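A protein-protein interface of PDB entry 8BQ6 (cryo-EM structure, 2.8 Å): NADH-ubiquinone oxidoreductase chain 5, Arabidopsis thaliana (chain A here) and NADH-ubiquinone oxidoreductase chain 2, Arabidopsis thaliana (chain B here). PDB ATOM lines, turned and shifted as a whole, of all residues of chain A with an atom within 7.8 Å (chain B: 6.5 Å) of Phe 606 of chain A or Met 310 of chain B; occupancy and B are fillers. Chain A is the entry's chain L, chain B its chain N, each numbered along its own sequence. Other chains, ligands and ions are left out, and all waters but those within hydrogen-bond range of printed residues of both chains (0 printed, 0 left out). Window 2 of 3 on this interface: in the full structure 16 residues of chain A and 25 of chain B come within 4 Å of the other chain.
Phe 606 of chain A touches just these residues of chain B: Leu 307 (3.7 Å), Met 310 (3.6 Å) and Ile 435 (3.5 Å). Met 310 of chain B touches just these residues of chain A: Phe 606 (3.6 Å) and Ala 610 (3.8 Å). No residue of chain A comes within 4 Å of Ala 309 of chain B. Of the printed residues of chain B, Ile 613 of chain A touches Ala 308. Of the printed residues of chain A, Ile 435 of chain B touches Phe 606 (3.5 Å). Printed residues of chain A within 4 Å of Leu 307 of chain B: Phe 606 and Ala 610. Tyr 321 of chain B touches none of the printed residues of chain A. Arg 608 of chain A touches none of the printed residues of chain B.
Of the 15 printed residues of chain A, 4 touch a printed residue of chain B. Along chain B the printed residues that touch a printed residue of chain A span positions 307 to 435. Among the printed residues, 8 pairs touch across the chains. Among the printed residues, no Asp or Glu carboxylate lies within 4 Å of a Lys or Arg side-chain nitrogen of the other chain.
Among the printed residues, merely in contact across the chains: Phe 606 of chain A with Leu 307 of chain B, Phe 606 of chain A with Met 310 of chain B, Phe 606 of chain A with Ile 435 of chain B, Ala 610 of chain A with Leu 307 of chain B, Ala 610 of chain A with Met 310 of chain B, Ala 610 of chain A with Ala 311 of chain B, Ile 613 of chain A with Ala 308 of chain B and Ser 614 of chain A with Ala 311 of chain B.
The backbone carbonyl oxygen of Ala 308 of chain B is in hydrogen-bond range of the side-chain amide nitrogen of Gln 312 of chain B (2.7 Å). NH2 of Arg 442 of chain B lies within hydrogen-bond range of O of Met 310 of chain B (2.8 Å).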
ATOM      1  N   TYR A 600     -35.909   7.624 -32.286  1.00  0.00           N
ATOM      2  CA  TYR A 600     -36.536   8.066 -31.044  1.00  0.00           C
ATOM      3  C   TYR A 600     -37.143   6.897 -30.281  1.00  0.00           C
ATOM      4  O   TYR A 600     -36.932   6.754 -29.071  1.00  0.00           O
ATOM      5  CB  TYR A 600     -37.596   9.121 -31.340  1.00  0.00           C
ATOM      6  CG  TYR A 600     -38.224   9.683 -30.096  1.00  0.00           C
ATOM      7  CD1 TYR A 600     -37.485  10.449 -29.207  1.00  0.00           C
ATOM      8  CD2 TYR A 600     -39.554   9.435 -29.802  1.00  0.00           C
ATOM      9  CE1 TYR A 600     -38.061  10.960 -28.064  1.00  0.00           C
ATOM     10  CE2 TYR A 600     -40.137   9.943 -28.666  1.00  0.00           C
ATOM     11  CZ  TYR A 600     -39.388  10.703 -27.800  1.00  0.00           C
ATOM     12  OH  TYR A 600     -39.972  11.206 -26.663  1.00  0.00           O
ATOM     13  N   GLY A 601     -37.915   6.057 -30.970  1.00  0.00           N
ATOM     14  CA  GLY A 601     -38.487   4.892 -30.320  1.00  0.00           C
ATOM     15  C   GLY A 601     -37.451   3.845 -29.958  1.00  0.00           C
ATOM     16  O   GLY A 601     -37.565   3.180 -28.927  1.00  0.00           O
ATOM     17  N   ILE A 602     -36.438   3.669 -30.812  1.00  0.00           N
ATOM     18  CA  ILE A 602     -35.431   2.635 -30.582  1.00  0.00           C
ATOM     19  C   ILE A 602     -34.600   2.958 -29.346  1.00  0.00           C
ATOM     20  O   ILE A 602     -34.258   2.066 -28.559  1.00  0.00           O
ATOM     21  CB  ILE A 602     -34.551   2.458 -31.834  1.00  0.00           C
ATOM     22  CG1 ILE A 602     -35.253   1.561 -32.855  1.00  0.00           C
ATOM     23  CG2 ILE A 602     -33.185   1.904 -31.477  1.00  0.00           C
ATOM     24  CD1 ILE A 602     -34.845   1.827 -34.273  1.00  0.00           C
ATOM     25  N   SER A 603     -34.253   4.232 -29.163  1.00  0.00           N
ATOM     26  CA  SER A 603     -33.535   4.630 -27.959  1.00  0.00           C
ATOM     27  C   SER A 603     -34.381   4.404 -26.714  1.00  0.00           C
ATOM     28  O   SER A 603     -33.875   3.943 -25.685  1.00  0.00           O
ATOM     29  CB  SER A 603     -33.114   6.095 -28.060  1.00  0.00           C
ATOM     30  OG  SER A 603     -34.244   6.947 -28.106  1.00  0.00           O
ATOM     31  N   TYR A 604     -35.674   4.718 -26.791  1.00  0.00           N
ATOM     32  CA  TYR A 604     -36.557   4.562 -25.639  1.00  0.00           C
ATOM     33  C   TYR A 604     -36.635   3.102 -25.193  1.00  0.00           C
ATOM     34  O   TYR A 604     -36.402   2.778 -24.016  1.00  0.00           O
ATOM     35  CB  TYR A 604     -37.949   5.078 -25.998  1.00  0.00           C
ATOM     36  CG  TYR A 604     -38.923   5.045 -24.855  1.00  0.00           C
ATOM     37  CD1 TYR A 604     -38.689   5.771 -23.698  1.00  0.00           C
ATOM     38  CD2 TYR A 604     -40.044   4.230 -24.905  1.00  0.00           C
ATOM     39  CE1 TYR A 604     -39.576   5.736 -22.650  1.00  0.00           C
ATOM     40  CE2 TYR A 604     -40.930   4.175 -23.854  1.00  0.00           C
ATOM     41  CZ  TYR A 604     -40.690   4.927 -22.727  1.00  0.00           C
ATOM     42  OH  TYR A 604     -41.575   4.876 -21.677  1.00  0.00           O
ATOM     43  N   THR A 605     -36.954   2.204 -26.129  1.00  0.00           N
ATOM     44  CA  THR A 605     -37.126   0.800 -25.772  1.00  0.00           C
ATOM     45  C   THR A 605     -35.821   0.192 -25.279  1.00  0.00           C
ATOM     46  O   THR A 605     -35.822  -0.612 -24.340  1.00  0.00           O
ATOM     47  CB  THR A 605     -37.675  -0.004 -26.953  1.00  0.00           C
ATOM     48  OG1 THR A 605     -37.599  -1.401 -26.650  1.00  0.00           O
ATOM     49  CG2 THR A 605     -36.877   0.251 -28.212  1.00  0.00           C
ATOM     50  N   PHE A 606     -34.696   0.557 -25.892  1.00  0.00           N
ATOM     51  CA  PHE A 606     -33.441  -0.041 -25.461  1.00  0.00           C
ATOM     52  C   PHE A 606     -32.974   0.537 -24.136  1.00  0.00           C
ATOM     53  O   PHE A 606     -32.326  -0.164 -23.357  1.00  0.00           O
ATOM     54  CB  PHE A 606     -32.386   0.106 -26.551  1.00  0.00           C
ATOM     55  CG  PHE A 606     -32.381  -1.042 -27.509  1.00  0.00           C
ATOM     56  CD1 PHE A 606     -31.838  -2.259 -27.145  1.00  0.00           C
ATOM     57  CD2 PHE A 606     -32.983  -0.927 -28.748  1.00  0.00           C
ATOM     58  CE1 PHE A 606     -31.855  -3.328 -28.019  1.00  0.00           C
ATOM     59  CE2 PHE A 606     -33.007  -1.991 -29.624  1.00  0.00           C
ATOM     60  CZ  PHE A 606     -32.444  -3.193 -29.260  1.00  0.00           C
ATOM     61  N   ARG A 607     -33.330   1.787 -23.839  1.00  0.00           N
ATOM     62  CA  ARG A 607     -33.054   2.330 -22.514  1.00  0.00           C
ATOM     63  C   ARG A 607     -33.837   1.575 -21.444  1.00  0.00           C
ATOM     64  O   ARG A 607     -33.294   1.243 -20.384  1.00  0.00           O
ATOM     65  CB  ARG A 607     -33.375   3.823 -22.484  1.00  0.00           C
ATOM     66  CG  ARG A 607     -32.249   4.695 -23.015  1.00  0.00           C
ATOM     67  CD  ARG A 607     -32.373   6.134 -22.556  1.00  0.00           C
ATOM     68  NE  ARG A 607     -33.207   6.925 -23.453  1.00  0.00           N
ATOM     69  CZ  ARG A 607     -34.371   7.456 -23.110  1.00  0.00           C
ATOM     70  NH1 ARG A 607     -34.869   7.300 -21.896  1.00  0.00           N
ATOM     71  NH2 ARG A 607     -35.049   8.166 -24.006  1.00  0.00           N
ATOM     72  N   ARG A 608     -35.116   1.277 -21.710  1.00  0.00           N
ATOM     73  CA  ARG A 608     -35.890   0.498 -20.740  1.00  0.00           C
ATOM     74  C   ARG A 608     -35.356  -0.924 -20.594  1.00  0.00           C
ATOM     75  O   ARG A 608     -35.295  -1.461 -19.480  1.00  0.00           O
ATOM     76  CB  ARG A 608     -37.368   0.457 -21.123  1.00  0.00           C
ATOM     77  CG  ARG A 608     -37.989   1.822 -21.184  1.00  0.00           C
ATOM     78  CD  ARG A 608     -38.150   2.365 -19.796  1.00  0.00           C
ATOM     79  NE  ARG A 608     -38.792   3.666 -19.814  1.00  0.00           N
ATOM     80  CZ  ARG A 608     -38.124   4.808 -19.861  1.00  0.00           C
ATOM     81  NH1 ARG A 608     -36.807   4.829 -19.963  1.00  0.00           N
ATOM     82  NH2 ARG A 608     -38.792   5.955 -19.791  1.00  0.00           N
ATOM     83  N   LEU A 609     -34.986  -1.553 -21.711  1.00  0.00           N
ATOM     84  CA  LEU A 609     -34.421  -2.897 -21.664  1.00  0.00           C
ATOM     85  C   LEU A 609     -33.118  -2.922 -20.872  1.00  0.00           C
ATOM     86  O   LEU A 609     -32.882  -3.841 -20.078  1.00  0.00           O
ATOM     87  CB  LEU A 609     -34.199  -3.407 -23.086  1.00  0.00           C
ATOM     88  CG  LEU A 609     -35.440  -3.826 -23.880  1.00  0.00           C
ATOM     89  CD1 LEU A 609     -35.038  -4.550 -25.152  1.00  0.00           C
ATOM     90  CD2 LEU A 609     -36.339  -4.706 -23.035  1.00  0.00           C
ATOM     91  N   ALA A 610     -32.259  -1.921 -21.080  1.00  0.00           N
ATOM     92  CA  ALA A 610     -31.018  -1.830 -20.319  1.00  0.00           C
ATOM     93  C   ALA A 610     -31.294  -1.598 -18.838  1.00  0.00           C
ATOM     94  O   ALA A 610     -30.622  -2.179 -17.978  1.00  0.00           O
ATOM     95  CB  ALA A 610     -30.138  -0.719 -20.892  1.00  0.00           C
ATOM     96  N   GLU A 611     -32.286  -0.762 -18.521  1.00  0.00           N
ATOM     97  CA  GLU A 611     -32.657  -0.542 -17.127  1.00  0.00           C
ATOM     98  C   GLU A 611     -33.119  -1.831 -16.458  1.00  0.00           C
ATOM     99  O   GLU A 611     -32.772  -2.107 -15.304  1.00  0.00           O
ATOM    100  CB  GLU A 611     -33.752   0.517 -17.036  1.00  0.00           C
ATOM    101  CG  GLU A 611     -33.830   1.172 -15.679  1.00  0.00           C
ATOM    102  CD  GLU A 611     -35.225   1.635 -15.332  1.00  0.00           C
ATOM    103  OE1 GLU A 611     -36.068   0.788 -14.969  1.00  0.00           O
ATOM    104  OE2 GLU A 611     -35.478   2.853 -15.415  1.00  0.00           O
ATOM    105  N   ARG A 612     -33.924  -2.625 -17.166  1.00  0.00           N
ATOM    106  CA  ARG A 612     -34.430  -3.866 -16.585  1.00  0.00           C
ATOM    107  C   ARG A 612     -33.327  -4.903 -16.429  1.00  0.00           C
ATOM    108  O   ARG A 612     -33.272  -5.612 -15.417  1.00  0.00           O
ATOM    109  CB  ARG A 612     -35.555  -4.429 -17.445  1.00  0.00           C
ATOM    110  CG  ARG A 612     -36.928  -3.942 -17.070  1.00  0.00           C
ATOM    111  CD  ARG A 612     -37.897  -4.133 -18.223  1.00  0.00           C
ATOM    112  NE  ARG A 612     -37.899  -5.500 -18.735  1.00  0.00           N
ATOM    113  CZ  ARG A 612     -38.926  -6.335 -18.650  1.00  0.00           C
ATOM    114  NH1 ARG A 612     -40.047  -5.993 -18.037  1.00  0.00           N
ATOM    115  NH2 ARG A 612     -38.824  -7.546 -19.188  1.00  0.00           N
ATOM    116  N   ILE A 613     -32.459  -5.031 -17.435  1.00  0.00           N
ATOM    117  CA  ILE A 613     -31.363  -5.993 -17.351  1.00  0.00           C
ATOM    118  C   ILE A 613     -30.400  -5.603 -16.237  1.00  0.00           C
ATOM    119  O   ILE A 613     -29.845  -6.467 -15.545  1.00  0.00           O
ATOM    120  CB  ILE A 613     -30.653  -6.110 -18.715  1.00  0.00           C
ATOM    121  CG1 ILE A 613     -31.158  -7.330 -19.486  1.00  0.00           C
ATOM    122  CG2 ILE A 613     -29.148  -6.183 -18.553  1.00  0.00           C
ATOM    123  CD1 ILE A 613     -32.636  -7.300 -19.783  1.00  0.00           C
ATOM    124  N   SER A 614     -30.200  -4.301 -16.035  1.00  0.00           N
ATOM    125  CA  SER A 614     -29.347  -3.838 -14.947  1.00  0.00           C
ATOM    126  C   SER A 614     -29.935  -4.201 -13.589  1.00  0.00           C
ATOM    127  O   SER A 614     -29.198  -4.506 -12.644  1.00  0.00           O
ATOM    128  CB  SER A 614     -29.139  -2.329 -15.065  1.00  0.00           C
ATOM    129  OG  SER A 614     -28.460  -1.806 -13.939  1.00  0.00           O
ATOM    130  N   GLY B 305     -24.713  -8.851 -22.112  1.00  0.00           N
ATOM    131  CA  GLY B 305     -23.573  -7.971 -21.951  1.00  0.00           C
ATOM    132  C   GLY B 305     -23.793  -6.626 -22.609  1.00  0.00           C
ATOM    133  O   GLY B 305     -23.513  -5.584 -22.014  1.00  0.00           O
ATOM    134  N   ALA B 306     -24.324  -6.627 -23.838  1.00  0.00           N
ATOM    135  CA  ALA B 306     -24.555  -5.359 -24.527  1.00  0.00           C
ATOM    136  C   ALA B 306     -25.540  -4.480 -23.762  1.00  0.00           C
ATOM    137  O   ALA B 306     -25.276  -3.293 -23.522  1.00  0.00           O
ATOM    138  CB  ALA B 306     -25.048  -5.618 -25.950  1.00  0.00           C
ATOM    139  N   LEU B 307     -26.675  -5.049 -23.347  1.00  0.00           N
ATOM    140  CA  LEU B 307     -27.674  -4.237 -22.651  1.00  0.00           C
ATOM    141  C   LEU B 307     -27.146  -3.725 -21.311  1.00  0.00           C
ATOM    142  O   LEU B 307     -27.255  -2.529 -20.992  1.00  0.00           O
ATOM    143  CB  LEU B 307     -28.960  -5.039 -22.454  1.00  0.00           C
ATOM    144  CG  LEU B 307     -29.735  -5.405 -23.722  1.00  0.00           C
ATOM    145  CD1 LEU B 307     -30.965  -6.214 -23.371  1.00  0.00           C
ATOM    146  CD2 LEU B 307     -30.122  -4.156 -24.494  1.00  0.00           C
ATOM    147  N   ALA B 308     -26.556  -4.619 -20.515  1.00  0.00           N
ATOM    148  CA  ALA B 308     -26.090  -4.230 -19.192  1.00  0.00           C
ATOM    149  C   ALA B 308     -24.973  -3.200 -19.275  1.00  0.00           C
ATOM    150  O   ALA B 308     -24.937  -2.254 -18.479  1.00  0.00           O
ATOM    151  CB  ALA B 308     -25.638  -5.462 -18.418  1.00  0.00           C
ATOM    152  N   ALA B 309     -24.048  -3.361 -20.226  1.00  0.00           N
ATOM    153  CA  ALA B 309     -23.018  -2.349 -20.412  1.00  0.00           C
ATOM    154  C   ALA B 309     -23.635  -1.016 -20.794  1.00  0.00           C
ATOM    155  O   ALA B 309     -23.227   0.033 -20.281  1.00  0.00           O
ATOM    156  CB  ALA B 309     -22.016  -2.803 -21.470  1.00  0.00           C
ATOM    157  N   MET B 310     -24.640  -1.035 -21.679  1.00  0.00           N
ATOM    158  CA  MET B 310     -25.326   0.202 -22.031  1.00  0.00           C
ATOM    159  C   MET B 310     -25.931   0.878 -20.806  1.00  0.00           C
ATOM    160  O   MET B 310     -26.059   2.107 -20.773  1.00  0.00           O
ATOM    161  CB  MET B 310     -26.405  -0.082 -23.074  1.00  0.00           C
ATOM    162  CG  MET B 310     -27.526   0.925 -23.082  1.00  0.00           C
ATOM    163  SD  MET B 310     -28.269   1.120 -24.703  1.00  0.00           S
ATOM    164  CE  MET B 310     -29.059  -0.472 -24.859  1.00  0.00           C
ATOM    165  N   ALA B 311     -26.292   0.101 -19.782  1.00  0.00           N
ATOM    166  CA  ALA B 311     -26.864   0.701 -18.579  1.00  0.00           C
ATOM    167  C   ALA B 311     -25.833   1.226 -17.571  1.00  0.00           C
ATOM    168  O   ALA B 311     -26.229   1.890 -16.609  1.00  0.00           O
ATOM    169  CB  ALA B 311     -27.772  -0.306 -17.877  1.00  0.00           C
ATOM    170  N   GLN B 312     -24.539   0.958 -17.749  1.00  0.00           N
ATOM    171  CA  GLN B 312     -23.558   1.270 -16.708  1.00  0.00           C
ATOM    172  C   GLN B 312     -23.099   2.728 -16.749  1.00  0.00           C
ATOM    173  O   GLN B 312     -22.995   3.333 -17.819  1.00  0.00           O
ATOM    174  CB  GLN B 312     -22.338   0.357 -16.832  1.00  0.00           C
ATOM    175  CG  GLN B 312     -22.595  -1.124 -16.582  1.00  0.00           C
ATOM    176  CD  GLN B 312     -23.573  -1.378 -15.452  1.00  0.00           C
ATOM    177  OE1 GLN B 312     -23.292  -1.078 -14.296  1.00  0.00           O
ATOM    178  NE2 GLN B 312     -24.717  -1.961 -15.780  1.00  0.00           N
ATOM    179  N   THR B 313     -22.805   3.285 -15.568  1.00  0.00           N
ATOM    180  CA  THR B 313     -22.215   4.616 -15.447  1.00  0.00           C
ATOM    181  C   THR B 313     -20.812   4.605 -14.853  1.00  0.00           C
ATOM    182  O   THR B 313     -20.208   5.674 -14.717  1.00  0.00           O
ATOM    183  CB  THR B 313     -23.094   5.543 -14.594  1.00  0.00           C
ATOM    184  OG1 THR B 313     -23.208   5.023 -13.263  1.00  0.00           O
ATOM    185  CG2 THR B 313     -24.474   5.700 -15.200  1.00  0.00           C
ATOM    186  N   LEU B 318     -18.593  -1.213 -16.753  1.00  0.00           N
ATOM    187  CA  LEU B 318     -18.677  -1.222 -18.205  1.00  0.00           C
ATOM    188  C   LEU B 318     -17.675  -2.207 -18.789  1.00  0.00           C
ATOM    189  O   LEU B 318     -18.007  -2.992 -19.684  1.00  0.00           O
ATOM    190  CB  LEU B 318     -18.441   0.185 -18.749  1.00  0.00           C
ATOM    191  CG  LEU B 318     -18.324   0.284 -20.263  1.00  0.00           C
ATOM    192  CD1 LEU B 318     -19.706   0.180 -20.870  1.00  0.00           C
ATOM    193  CD2 LEU B 318     -17.665   1.585 -20.642  1.00  0.00           C
ATOM    194  N   TYR B 321     -18.887  -5.908 -18.167  1.00  0.00           N
ATOM    195  CA  TYR B 321     -19.941  -6.324 -19.087  1.00  0.00           C
ATOM    196  C   TYR B 321     -19.428  -6.453 -20.515  1.00  0.00           C
ATOM    197  O   TYR B 321     -19.880  -7.331 -21.265  1.00  0.00           O
ATOM    198  CB  TYR B 321     -21.100  -5.342 -19.007  1.00  0.00           C
ATOM    199  CG  TYR B 321     -21.963  -5.600 -17.804  1.00  0.00           C
ATOM    200  CD1 TYR B 321     -22.598  -6.820 -17.638  1.00  0.00           C
ATOM    201  CD2 TYR B 321     -22.092  -4.651 -16.806  1.00  0.00           C
ATOM    202  CE1 TYR B 321     -23.373  -7.067 -16.531  1.00  0.00           C
ATOM    203  CE2 TYR B 321     -22.857  -4.891 -15.693  1.00  0.00           C
ATOM    204  CZ  TYR B 321     -23.500  -6.098 -15.562  1.00  0.00           C
ATOM    205  OH  TYR B 321     -24.269  -6.332 -14.451  1.00  0.00           O
ATOM    206  N   VAL B 431     -27.154  -6.497 -34.087  1.00  0.00           N
ATOM    207  CA  VAL B 431     -27.812  -5.601 -33.138  1.00  0.00           C
ATOM    208  C   VAL B 431     -26.897  -5.325 -31.945  1.00  0.00           C
ATOM    209  O   VAL B 431     -26.747  -4.176 -31.503  1.00  0.00           O
ATOM    210  CB  VAL B 431     -29.164  -6.180 -32.692  1.00  0.00           C
ATOM    211  CG1 VAL B 431     -29.785  -5.293 -31.627  1.00  0.00           C
ATOM    212  CG2 VAL B 431     -30.093  -6.363 -33.885  1.00  0.00           C
ATOM    213  N   ILE B 435     -25.211  -1.838 -30.459  1.00  0.00           N
ATOM    214  CA  ILE B 435     -25.348  -1.395 -29.070  1.00  0.00           C
ATOM    215  C   ILE B 435     -23.978  -1.170 -28.434  1.00  0.00           C
ATOM    216  O   ILE B 435     -23.748  -0.172 -27.728  1.00  0.00           O
ATOM    217  CB  ILE B 435     -26.177  -2.411 -28.267  1.00  0.00           C
ATOM    218  CG1 ILE B 435     -27.613  -2.446 -28.783  1.00  0.00           C
ATOM    219  CG2 ILE B 435     -26.147  -2.069 -26.790  1.00  0.00           C
ATOM    220  CD1 ILE B 435     -28.356  -3.690 -28.392  1.00  0.00           C
ATOM    221  N   PHE B 438     -22.427   1.986 -29.555  1.00  0.00           N
ATOM    222  CA  PHE B 438     -22.998   3.145 -28.873  1.00  0.00           C
ATOM    223  C   PHE B 438     -22.357   3.354 -27.506  1.00  0.00           C
ATOM    224  O   PHE B 438     -21.894   4.459 -27.182  1.00  0.00           O
ATOM    225  CB  PHE B 438     -24.506   2.990 -28.716  1.00  0.00           C
ATOM    226  CG  PHE B 438     -25.107   3.978 -27.760  1.00  0.00           C
ATOM    227  CD1 PHE B 438     -25.166   5.318 -28.095  1.00  0.00           C
ATOM    228  CD2 PHE B 438     -25.594   3.578 -26.529  1.00  0.00           C
ATOM    229  CE1 PHE B 438     -25.707   6.239 -27.234  1.00  0.00           C
ATOM    230  CE2 PHE B 438     -26.139   4.502 -25.657  1.00  0.00           C
ATOM    231  CZ  PHE B 438     -26.195   5.835 -26.012  1.00  0.00           C
ATOM    232  N   TYR B 439     -22.333   2.312 -26.677  1.00  0.00           N
ATOM    233  CA  TYR B 439     -21.830   2.584 -25.334  1.00  0.00           C
ATOM    234  C   TYR B 439     -20.311   2.715 -25.287  1.00  0.00           C
ATOM    235  O   TYR B 439     -19.785   3.212 -24.287  1.00  0.00           O
ATOM    236  CB  TYR B 439     -22.348   1.551 -24.318  1.00  0.00           C
ATOM    237  CG  TYR B 439     -21.856   0.130 -24.441  1.00  0.00           C
ATOM    238  CD1 TYR B 439     -20.542  -0.209 -24.158  1.00  0.00           C
ATOM    239  CD2 TYR B 439     -22.727  -0.880 -24.813  1.00  0.00           C
ATOM    240  CE1 TYR B 439     -20.111  -1.510 -24.261  1.00  0.00           C
ATOM    241  CE2 TYR B 439     -22.308  -2.175 -24.916  1.00  0.00           C
ATOM    242  CZ  TYR B 439     -20.998  -2.488 -24.649  1.00  0.00           C
ATOM    243  OH  TYR B 439     -20.587  -3.793 -24.757  1.00  0.00           O
ATOM    244  N   ARG B 442     -19.837   6.500 -26.409  1.00  0.00           N
ATOM    245  CA  ARG B 442     -20.241   7.414 -25.342  1.00  0.00           C
ATOM    246  C   ARG B 442     -19.040   7.901 -24.531  1.00  0.00           C
ATOM    247  O   ARG B 442     -19.012   9.051 -24.073  1.00  0.00           O
ATOM    248  CB  ARG B 442     -21.257   6.739 -24.432  1.00  0.00           C
ATOM    249  CG  ARG B 442     -22.004   7.703 -23.553  1.00  0.00           C
ATOM    250  CD  ARG B 442     -23.407   7.228 -23.314  1.00  0.00           C
ATOM    251  NE  ARG B 442     -23.394   5.909 -22.699  1.00  0.00           N
ATOM    252  CZ  ARG B 442     -24.468   5.289 -22.234  1.00  0.00           C
ATOM    253  NH1 ARG B 442     -25.658   5.866 -22.249  1.00  0.00           N
ATOM    254  NH2 ARG B 442     -24.343   4.064 -21.733  1.00  0.00           N
